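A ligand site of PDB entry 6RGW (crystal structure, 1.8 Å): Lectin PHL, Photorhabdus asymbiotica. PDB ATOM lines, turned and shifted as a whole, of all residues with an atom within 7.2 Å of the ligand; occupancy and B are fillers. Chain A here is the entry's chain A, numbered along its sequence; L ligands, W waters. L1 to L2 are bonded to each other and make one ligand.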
ATOM      1  N   ASP A  51      -2.663 -34.638  14.360  1.00  0.00           N
ATOM      2  CA  ASP A  51      -3.113 -33.281  14.769  1.00  0.00           C
ATOM      3  C   ASP A  51      -2.302 -32.785  15.978  1.00  0.00           C
ATOM      4  O   ASP A  51      -2.563 -31.652  16.409  1.00  0.00           O
ATOM      5  CB  ASP A  51      -4.618 -33.273  15.055  1.00  0.00           C
ATOM      6  CG  ASP A  51      -5.099 -34.211  16.164  1.00  0.00           C
ATOM      7  OD1 ASP A  51      -4.335 -35.154  16.520  1.00  0.00           O
ATOM      8  OD2 ASP A  51      -6.245 -34.010  16.651  1.00  0.00           O
ATOM      9  N   LYS A  52      -1.359 -33.592  16.489  1.00  0.00           N
ATOM     10  CA  LYS A  52      -0.471 -33.261  17.639  1.00  0.00           C
ATOM     11  C   LYS A  52      -1.284 -33.206  18.951  1.00  0.00           C
ATOM     12  O   LYS A  52      -0.718 -32.739  19.960  1.00  0.00           O
ATOM     13  CB  LYS A  52       0.287 -31.952  17.407  1.00  0.00           C
ATOM     14  CG  LYS A  52       1.189 -31.978  16.182  1.00  0.00           C
ATOM     15  CD  LYS A  52       2.288 -30.940  16.201  1.00  0.00           C
ATOM     16  CE  LYS A  52       3.059 -30.930  14.898  1.00  0.00           C
ATOM     17  NZ  LYS A  52       4.072 -29.854  14.853  1.00  0.00           N
ATOM     18  N   ALA A  53      -2.529 -33.705  18.948  1.00  0.00           N
ATOM     19  CA  ALA A  53      -3.314 -33.875  20.193  1.00  0.00           C
ATOM     20  C   ALA A  53      -2.930 -35.207  20.850  1.00  0.00           C
ATOM     21  O   ALA A  53      -2.397 -36.090  20.162  1.00  0.00           O
ATOM     22  CB  ALA A  53      -4.797 -33.825  19.909  1.00  0.00           C
ATOM     23  N   VAL A  54      -3.165 -35.314  22.150  1.00  0.00           N
ATOM     24  CA  VAL A  54      -2.989 -36.580  22.900  1.00  0.00           C
ATOM     25  C   VAL A  54      -4.305 -37.335  22.791  1.00  0.00           C
ATOM     26  O   VAL A  54      -5.353 -36.724  23.054  1.00  0.00           O
ATOM     27  CB  VAL A  54      -2.574 -36.324  24.364  1.00  0.00           C
ATOM     28  CG1 VAL A  54      -2.463 -37.629  25.132  1.00  0.00           C
ATOM     29  CG2 VAL A  54      -1.275 -35.533  24.449  1.00  0.00           C
ATOM     30  N   SER A  73      -9.839 -38.103  21.967  1.00  0.00           N
ATOM     31  CA  SER A  73      -8.844 -37.008  22.086  1.00  0.00           C
ATOM     32  C   SER A  73      -8.937 -36.353  23.462  1.00  0.00           C
ATOM     33  O   SER A  73     -10.061 -36.052  23.926  1.00  0.00           O
ATOM     34  CB  SER A  73      -9.040 -36.002  20.986  1.00  0.00           C
ATOM     35  OG  SER A  73      -8.125 -34.929  21.158  1.00  0.00           O
ATOM     36  N   LEU A  74      -7.793 -36.124  24.097  1.00  0.00           N
ATOM     37  CA  LEU A  74      -7.659 -35.241  25.285  1.00  0.00           C
ATOM     38  C   LEU A  74      -7.252 -33.845  24.811  1.00  0.00           C
ATOM     39  O   LEU A  74      -7.044 -32.967  25.669  1.00  0.00           O
ATOM     40  CB  LEU A  74      -6.605 -35.817  26.236  1.00  0.00           C
ATOM     41  CG  LEU A  74      -6.950 -37.163  26.871  1.00  0.00           C
ATOM     42  CD1 LEU A  74      -5.818 -37.623  27.783  1.00  0.00           C
ATOM     43  CD2 LEU A  74      -8.256 -37.094  27.637  1.00  0.00           C
ATOM     44  N   LYS A  75      -7.149 -33.641  23.489  1.00  0.00           N
ATOM     45  CA  LYS A  75      -6.747 -32.351  22.869  1.00  0.00           C
ATOM     46  C   LYS A  75      -5.307 -32.033  23.274  1.00  0.00           C
ATOM     47  O   LYS A  75      -4.515 -32.985  23.423  1.00  0.00           O
ATOM     48  CB  LYS A  75      -7.741 -31.246  23.261  1.00  0.00           C
ATOM     49  CG  LYS A  75      -9.200 -31.526  22.915  1.00  0.00           C
ATOM     50  CD  LYS A  75     -10.144 -30.512  23.525  1.00  0.00           C
ATOM     51  CE  LYS A  75     -11.414 -30.315  22.727  1.00  0.00           C
ATOM     52  NZ  LYS A  75     -12.295 -29.298  23.346  1.00  0.00           N
ATOM     53  N   GLY A  76      -4.977 -30.754  23.437  1.00  0.00           N
ATOM     54  CA  GLY A  76      -3.591 -30.287  23.621  1.00  0.00           C
ATOM     55  C   GLY A  76      -2.842 -30.292  22.305  1.00  0.00           C
ATOM     56  O   GLY A  76      -3.374 -30.797  21.303  1.00  0.00           O
ATOM     57  N   GLN A  77      -1.643 -29.710  22.305  1.00  0.00           N
ATOM     58  CA  GLN A  77      -0.720 -29.691  21.144  1.00  0.00           C
ATOM     59  C   GLN A  77       0.662 -29.965  21.726  1.00  0.00           C
ATOM     60  O   GLN A  77       1.173 -29.098  22.461  1.00  0.00           O
ATOM     61  CB  GLN A  77      -0.806 -28.345  20.402  1.00  0.00           C
ATOM     62  CG  GLN A  77      -2.139 -28.134  19.695  1.00  0.00           C
ATOM     63  CD  GLN A  77      -2.283 -28.994  18.464  1.00  0.00           C
ATOM     64  OE1 GLN A  77      -1.787 -28.646  17.389  1.00  0.00           O
ATOM     65  NE2 GLN A  77      -2.979 -30.111  18.597  1.00  0.00           N
ATOM     66  N   VAL A  78       1.201 -31.164  21.483  1.00  0.00           N
ATOM     67  CA  VAL A  78       2.381 -31.682  22.216  1.00  0.00           C
ATOM     68  C   VAL A  78       3.531 -31.951  21.244  1.00  0.00           C
ATOM     69  O   VAL A  78       3.262 -32.317  20.069  1.00  0.00           O
ATOM     70  CB  VAL A  78       2.041 -32.937  23.047  1.00  0.00           C
ATOM     71  CG1 VAL A  78       0.924 -32.652  24.031  1.00  0.00           C
ATOM     72  CG2 VAL A  78       1.705 -34.143  22.187  1.00  0.00           C
ATOM     73  N   THR A  79       4.756 -31.833  21.757  1.00  0.00           N
ATOM     74  CA  THR A  79       6.039 -32.060  21.040  1.00  0.00           C
ATOM     75  C   THR A  79       6.927 -33.031  21.836  1.00  0.00           C
ATOM     76  O   THR A  79       8.166 -32.999  21.655  1.00  0.00           O
ATOM     77  CB  THR A  79       6.706 -30.714  20.767  1.00  0.00           C
ATOM     78  OG1 THR A  79       6.970 -30.090  22.032  1.00  0.00           O
ATOM     79  CG2 THR A  79       5.852 -29.799  19.923  1.00  0.00           C
ATOM     80  N   ALA A  96       3.379 -33.898  29.199  1.00  0.00           N
ATOM     81  CA  ALA A  96       3.862 -33.743  27.820  1.00  0.00           C
ATOM     82  C   ALA A  96       4.506 -32.369  27.649  1.00  0.00           C
ATOM     83  O   ALA A  96       4.030 -31.406  28.284  1.00  0.00           O
ATOM     84  CB  ALA A  96       2.727 -33.927  26.850  1.00  0.00           C
ATOM     85  N   ARG A  97       5.507 -32.288  26.778  1.00  0.00           N
ATOM     86  CA  ARG A  97       6.008 -30.982  26.293  1.00  0.00           C
ATOM     87  C   ARG A  97       4.974 -30.396  25.343  1.00  0.00           C
ATOM     88  O   ARG A  97       4.473 -31.153  24.479  1.00  0.00           O
ATOM     89  CB  ARG A  97       7.363 -31.113  25.598  1.00  0.00           C
ATOM     90  CG  ARG A  97       7.993 -29.772  25.297  1.00  0.00           C
ATOM     91  CD  ARG A  97       9.379 -29.912  24.705  1.00  0.00           C
ATOM     92  NE  ARG A  97       9.358 -30.519  23.381  1.00  0.00           N
ATOM     93  CZ  ARG A  97      10.416 -30.630  22.593  1.00  0.00           C
ATOM     94  NH1 ARG A  97      11.590 -30.158  22.991  1.00  0.00           N
ATOM     95  NH2 ARG A  97      10.309 -31.203  21.411  1.00  0.00           N
ATOM     96  N   GLY A  98       4.651 -29.115  25.509  1.00  0.00           N
ATOM     97  CA  GLY A  98       3.756 -28.358  24.627  1.00  0.00           C
ATOM     98  C   GLY A  98       4.535 -27.830  23.431  1.00  0.00           C
ATOM     99  O   GLY A  98       5.768 -27.887  23.447  1.00  0.00           O
ATOM    100  N   THR A  99       3.827 -27.367  22.398  1.00  0.00           N
ATOM    101  CA  THR A  99       4.429 -26.672  21.226  1.00  0.00           C
ATOM    102  C   THR A  99       5.195 -25.432  21.704  1.00  0.00           C
ATOM    103  O   THR A  99       6.089 -24.995  20.940  1.00  0.00           O
ATOM    104  CB  THR A  99       3.356 -26.386  20.163  1.00  0.00           C
ATOM    105  OG1 THR A  99       2.240 -25.756  20.797  1.00  0.00           O
ATOM    106  CG2 THR A  99       2.886 -27.632  19.440  1.00  0.00           C
ATOM    107  N   ASP A 100       4.907 -24.908  22.896  1.00  0.00           N
ATOM    108  CA  ASP A 100       5.632 -23.752  23.501  1.00  0.00           C
ATOM    109  C   ASP A 100       6.881 -24.210  24.284  1.00  0.00           C
ATOM    110  O   ASP A 100       7.529 -23.344  24.894  1.00  0.00           O
ATOM    111  CB  ASP A 100       4.711 -22.898  24.379  1.00  0.00           C
ATOM    112  CG  ASP A 100       4.207 -23.594  25.631  1.00  0.00           C
ATOM    113  OD1 ASP A 100       4.512 -24.800  25.784  1.00  0.00           O
ATOM    114  OD2 ASP A 100       3.535 -22.929  26.433  1.00  0.00           O
ATOM    115  N   ASN A 101       7.186 -25.513  24.271  1.00  0.00           N
ATOM    116  CA  ASN A 101       8.357 -26.151  24.932  1.00  0.00           C
ATOM    117  C   ASN A 101       8.236 -26.126  26.470  1.00  0.00           C
ATOM    118  O   ASN A 101       9.212 -26.532  27.136  1.00  0.00           O
ATOM    119  CB  ASN A 101       9.671 -25.530  24.465  1.00  0.00           C
ATOM    120  CG  ASN A 101       9.988 -25.919  23.049  1.00  0.00           C
ATOM    121  OD1 ASN A 101       9.943 -27.102  22.709  1.00  0.00           O
ATOM    122  ND2 ASN A 101      10.276 -24.935  22.205  1.00  0.00           N
ATOM    123  N   ALA A 102       7.105 -25.715  27.028  1.00  0.00           N
ATOM    124  CA  ALA A 102       6.852 -25.843  28.483  1.00  0.00           C
ATOM    125  C   ALA A 102       6.414 -27.269  28.798  1.00  0.00           C
ATOM    126  O   ALA A 102       6.043 -28.037  27.875  1.00  0.00           O
ATOM    127  CB  ALA A 102       5.859 -24.825  28.956  1.00  0.00           C
ATOM    128  N   LEU A 103       6.482 -27.639  30.075  1.00  0.00           N
ATOM    129  CA  LEU A 103       5.859 -28.879  30.576  1.00  0.00           C
ATOM    130  C   LEU A 103       4.381 -28.577  30.814  1.00  0.00           C
ATOM    131  O   LEU A 103       4.064 -27.609  31.530  1.00  0.00           O
ATOM    132  CB  LEU A 103       6.549 -29.347  31.864  1.00  0.00           C
ATOM    133  CG  LEU A 103       5.858 -30.530  32.549  1.00  0.00           C
ATOM    134  CD1 LEU A 103       5.955 -31.775  31.695  1.00  0.00           C
ATOM    135  CD2 LEU A 103       6.454 -30.771  33.931  1.00  0.00           C
ATOM    136  N   TRP A 104       3.521 -29.408  30.225  1.00  0.00           N
ATOM    137  CA  TRP A 104       2.053 -29.329  30.413  1.00  0.00           C
ATOM    138  C   TRP A 104       1.582 -30.614  31.097  1.00  0.00           C
ATOM    139  O   TRP A 104       2.249 -31.652  30.965  1.00  0.00           O
ATOM    140  CB  TRP A 104       1.344 -29.134  29.068  1.00  0.00           C
ATOM    141  CG  TRP A 104       1.518 -27.756  28.501  1.00  0.00           C
ATOM    142  CD1 TRP A 104       2.627 -27.259  27.903  1.00  0.00           C
ATOM    143  CD2 TRP A 104       0.548 -26.703  28.504  1.00  0.00           C
ATOM    144  NE1 TRP A 104       2.414 -25.964  27.521  1.00  0.00           N
ATOM    145  CE2 TRP A 104       1.150 -25.587  27.874  1.00  0.00           C
ATOM    146  CE3 TRP A 104      -0.775 -26.577  28.959  1.00  0.00           C
ATOM    147  CZ2 TRP A 104       0.472 -24.379  27.694  1.00  0.00           C
ATOM    148  CZ3 TRP A 104      -1.442 -25.382  28.781  1.00  0.00           C
ATOM    149  CH2 TRP A 104      -0.827 -24.301  28.152  1.00  0.00           C
ATOM    150  N   HIS A 105       0.440 -30.550  31.765  1.00  0.00           N
ATOM    151  CA  HIS A 105      -0.169 -31.773  32.342  1.00  0.00           C
ATOM    152  C   HIS A 105      -1.690 -31.648  32.335  1.00  0.00           C
ATOM    153  O   HIS A 105      -2.209 -30.532  32.208  1.00  0.00           O
ATOM    154  CB  HIS A 105       0.439 -32.089  33.716  1.00  0.00           C
ATOM    155  CG  HIS A 105       0.106 -31.122  34.792  1.00  0.00           C
ATOM    156  ND1 HIS A 105      -0.190 -31.531  36.075  1.00  0.00           N
ATOM    157  CD2 HIS A 105       0.012 -29.774  34.801  1.00  0.00           C
ATOM    158  CE1 HIS A 105      -0.441 -30.484  36.829  1.00  0.00           C
ATOM    159  NE2 HIS A 105      -0.326 -29.384  36.062  1.00  0.00           N
ATOM    160  N   ASN A 117      -8.713 -29.565  32.479  1.00  0.00           N
ATOM    161  CA  ASN A 117      -8.126 -28.911  31.278  1.00  0.00           C
ATOM    162  C   ASN A 117      -6.605 -29.051  31.380  1.00  0.00           C
ATOM    163  O   ASN A 117      -6.093 -29.260  32.510  1.00  0.00           O
ATOM    164  CB  ASN A 117      -8.573 -27.465  31.133  1.00  0.00           C
ATOM    165  CG  ASN A 117     -10.047 -27.360  30.806  1.00  0.00           C
ATOM    166  OD1 ASN A 117     -10.515 -27.957  29.845  1.00  0.00           O
ATOM    167  ND2 ASN A 117     -10.781 -26.631  31.622  1.00  0.00           N
ATOM    168  N   TRP A 118      -5.926 -28.971  30.238  1.00  0.00           N
ATOM    169  CA  TRP A 118      -4.446 -28.878  30.195  1.00  0.00           C
ATOM    170  C   TRP A 118      -4.025 -27.640  30.983  1.00  0.00           C
ATOM    171  O   TRP A 118      -4.685 -26.593  30.853  1.00  0.00           O
ATOM    172  CB  TRP A 118      -3.952 -28.815  28.754  1.00  0.00           C
ATOM    173  CG  TRP A 118      -3.976 -30.126  28.043  1.00  0.00           C
ATOM    174  CD1 TRP A 118      -4.929 -30.603  27.188  1.00  0.00           C
ATOM    175  CD2 TRP A 118      -2.953 -31.138  28.106  1.00  0.00           C
ATOM    176  NE1 TRP A 118      -4.561 -31.829  26.706  1.00  0.00           N
ATOM    177  CE2 TRP A 118      -3.364 -32.191  27.263  1.00  0.00           C
ATOM    178  CE3 TRP A 118      -1.740 -31.265  28.794  1.00  0.00           C
ATOM    179  CZ2 TRP A 118      -2.600 -33.336  27.087  1.00  0.00           C
ATOM    180  CZ3 TRP A 118      -0.985 -32.401  28.625  1.00  0.00           C
ATOM    181  CH2 TRP A 118      -1.410 -33.414  27.771  1.00  0.00           C
ATOM    182  N   GLN A 119      -2.979 -27.767  31.801  1.00  0.00           N
ATOM    183  CA  GLN A 119      -2.390 -26.655  32.576  1.00  0.00           C
ATOM    184  C   GLN A 119      -0.872 -26.682  32.346  1.00  0.00           C
ATOM    185  O   GLN A 119      -0.309 -27.775  32.244  1.00  0.00           O
ATOM    186  CB  GLN A 119      -2.782 -26.776  34.055  1.00  0.00           C
ATOM    187  CG  GLN A 119      -2.086 -25.779  34.975  1.00  0.00           C
ATOM    188  CD  GLN A 119      -2.163 -26.154  36.433  1.00  0.00           C
ATOM    189  OE1 GLN A 119      -1.260 -26.780  36.990  1.00  0.00           O
ATOM    190  NE2 GLN A 119      -3.257 -25.760  37.065  1.00  0.00           N
HETATM  191  C1  LIG L   1      -2.286 -25.239  23.192  1.00  0.00           C
HETATM  192  C2  LIG L   1      -1.573 -23.907  23.340  1.00  0.00           C
HETATM  193  O1  LIG L   1      -2.097 -22.949  22.418  1.00  0.00           O
HETATM  194  O2  LIG L   1      -1.773 -26.136  24.172  1.00  0.00           O
HETATM  195  C3  LIG L   1      -0.403 -26.469  23.944  1.00  0.00           C
HETATM  196  C4  LIG L   1       0.469 -25.205  24.007  1.00  0.00           C
HETATM  197  O3  LIG L   1       1.821 -25.497  23.655  1.00  0.00           O
HETATM  198  C5  LIG L   1      -0.086 -24.122  23.065  1.00  0.00           C
HETATM  199  O4  LIG L   1       0.604 -22.885  23.225  1.00  0.00           O
HETATM  200  C6  LIG L   1      -0.012 -27.507  24.993  1.00  0.00           C
HETATM  201  O5  LIG L   1      -0.839 -28.669  24.834  1.00  0.00           O
HETATM  202  C7  LIG L   1       1.253 -22.457  22.019  1.00  0.00           C
HETATM  203  C8  LIG L   1      -0.702 -29.584  25.915  1.00  0.00           C
HETATM  204  C1  LG2 L   2      -7.215 -27.124  23.396  1.00  0.00           C
HETATM  205  C2  LG2 L   2      -6.402 -27.077  22.103  1.00  0.00           C
HETATM  206  C3  LG2 L   2      -5.300 -26.008  22.195  1.00  0.00           C
HETATM  207  C4  LG2 L   2      -4.475 -26.192  23.461  1.00  0.00           C
HETATM  208  C5  LG2 L   2      -5.378 -26.296  24.699  1.00  0.00           C
HETATM  209  C6  LG2 L   2      -4.571 -26.544  25.959  1.00  0.00           C
HETATM  210  O1  LG2 L   2      -5.852 -28.392  21.889  1.00  0.00           O
HETATM  211  O2  LG2 L   2      -4.453 -26.046  21.045  1.00  0.00           O
HETATM  212  O3  LG2 L   2      -3.568 -25.084  23.653  1.00  0.00           O
HETATM  213  O4  LG2 L   2      -6.338 -27.357  24.509  1.00  0.00           O
HETATM  214  C7  LG2 L   2      -6.055 -28.967  20.589  1.00  0.00           C
HETATM  215  C8  LG2 L   2      -5.124 -25.802  19.797  1.00  0.00           C
HETATM  216  O5  LG2 L   2      -7.931 -25.896  23.580  1.00  0.00           O
HETATM  217  O   HOH W   1      -0.450 -21.000  25.960  1.00  0.00           O
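Residues that only touch the ligand: Trp 118 (3.5 Å), Gly 98 (3.6 Å), Trp 104 (3.6 Å), Lys 75 (3.7 Å) and Val 78 (3.95 Å).
NE2 of Gln 77 sits at hydrogen-bond distance from O of Asp 51 (2.7 Å).
The backbone carbonyl oxygen (O) of Gly 98 sits at hydrogen-bond distance from the side-chain hydroxyl (OG1) of Thr 79 (2.9 Å).
OG of Ser 73 is in hydrogen-bond range of N of Lys 75 (2.8 Å).
The backbone NH (N) of Thr 99 sits at hydrogen-bond distance from the backbone carbonyl oxygen (O) of Gln 77.
The backbone carbonyl oxygen of Lys 75 lies within hydrogen-bond range of the backbone NH of Val 54 (3.0 Å).
The side-chain carboxylate (OD1) of Asp 100 is in hydrogen-bond range of the backbone NH (N) of Ala 102 (3.0 Å).
The backbone carbonyl oxygen of Lys 75 is in hydrogen-bond range of the indole nitrogen of Trp 118 (3.5 Å).
The indole nitrogen (NE1) of Trp 104 lies within hydrogen-bond range of the side-chain carboxylate (OD1) of Asp 100.
N of Gln 77 sits at hydrogen-bond distance from O5 of LIG L1, at 2.9 Å.
N of Asp 100 is in hydrogen-bond range of O3 of LIG L1 (3.2 Å).
The backbone NH of Gly 76 lies within hydrogen-bond range of an oxygen (O1) of LG2 L2 (3.0 Å).
The backbone NH of Thr 99 is in hydrogen-bond range of an oxygen (O3) of LIG L1 (3.0 Å).
OG1 of Thr 99 is in hydrogen-bond range of O3 of LIG L1 (2.9 Å).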
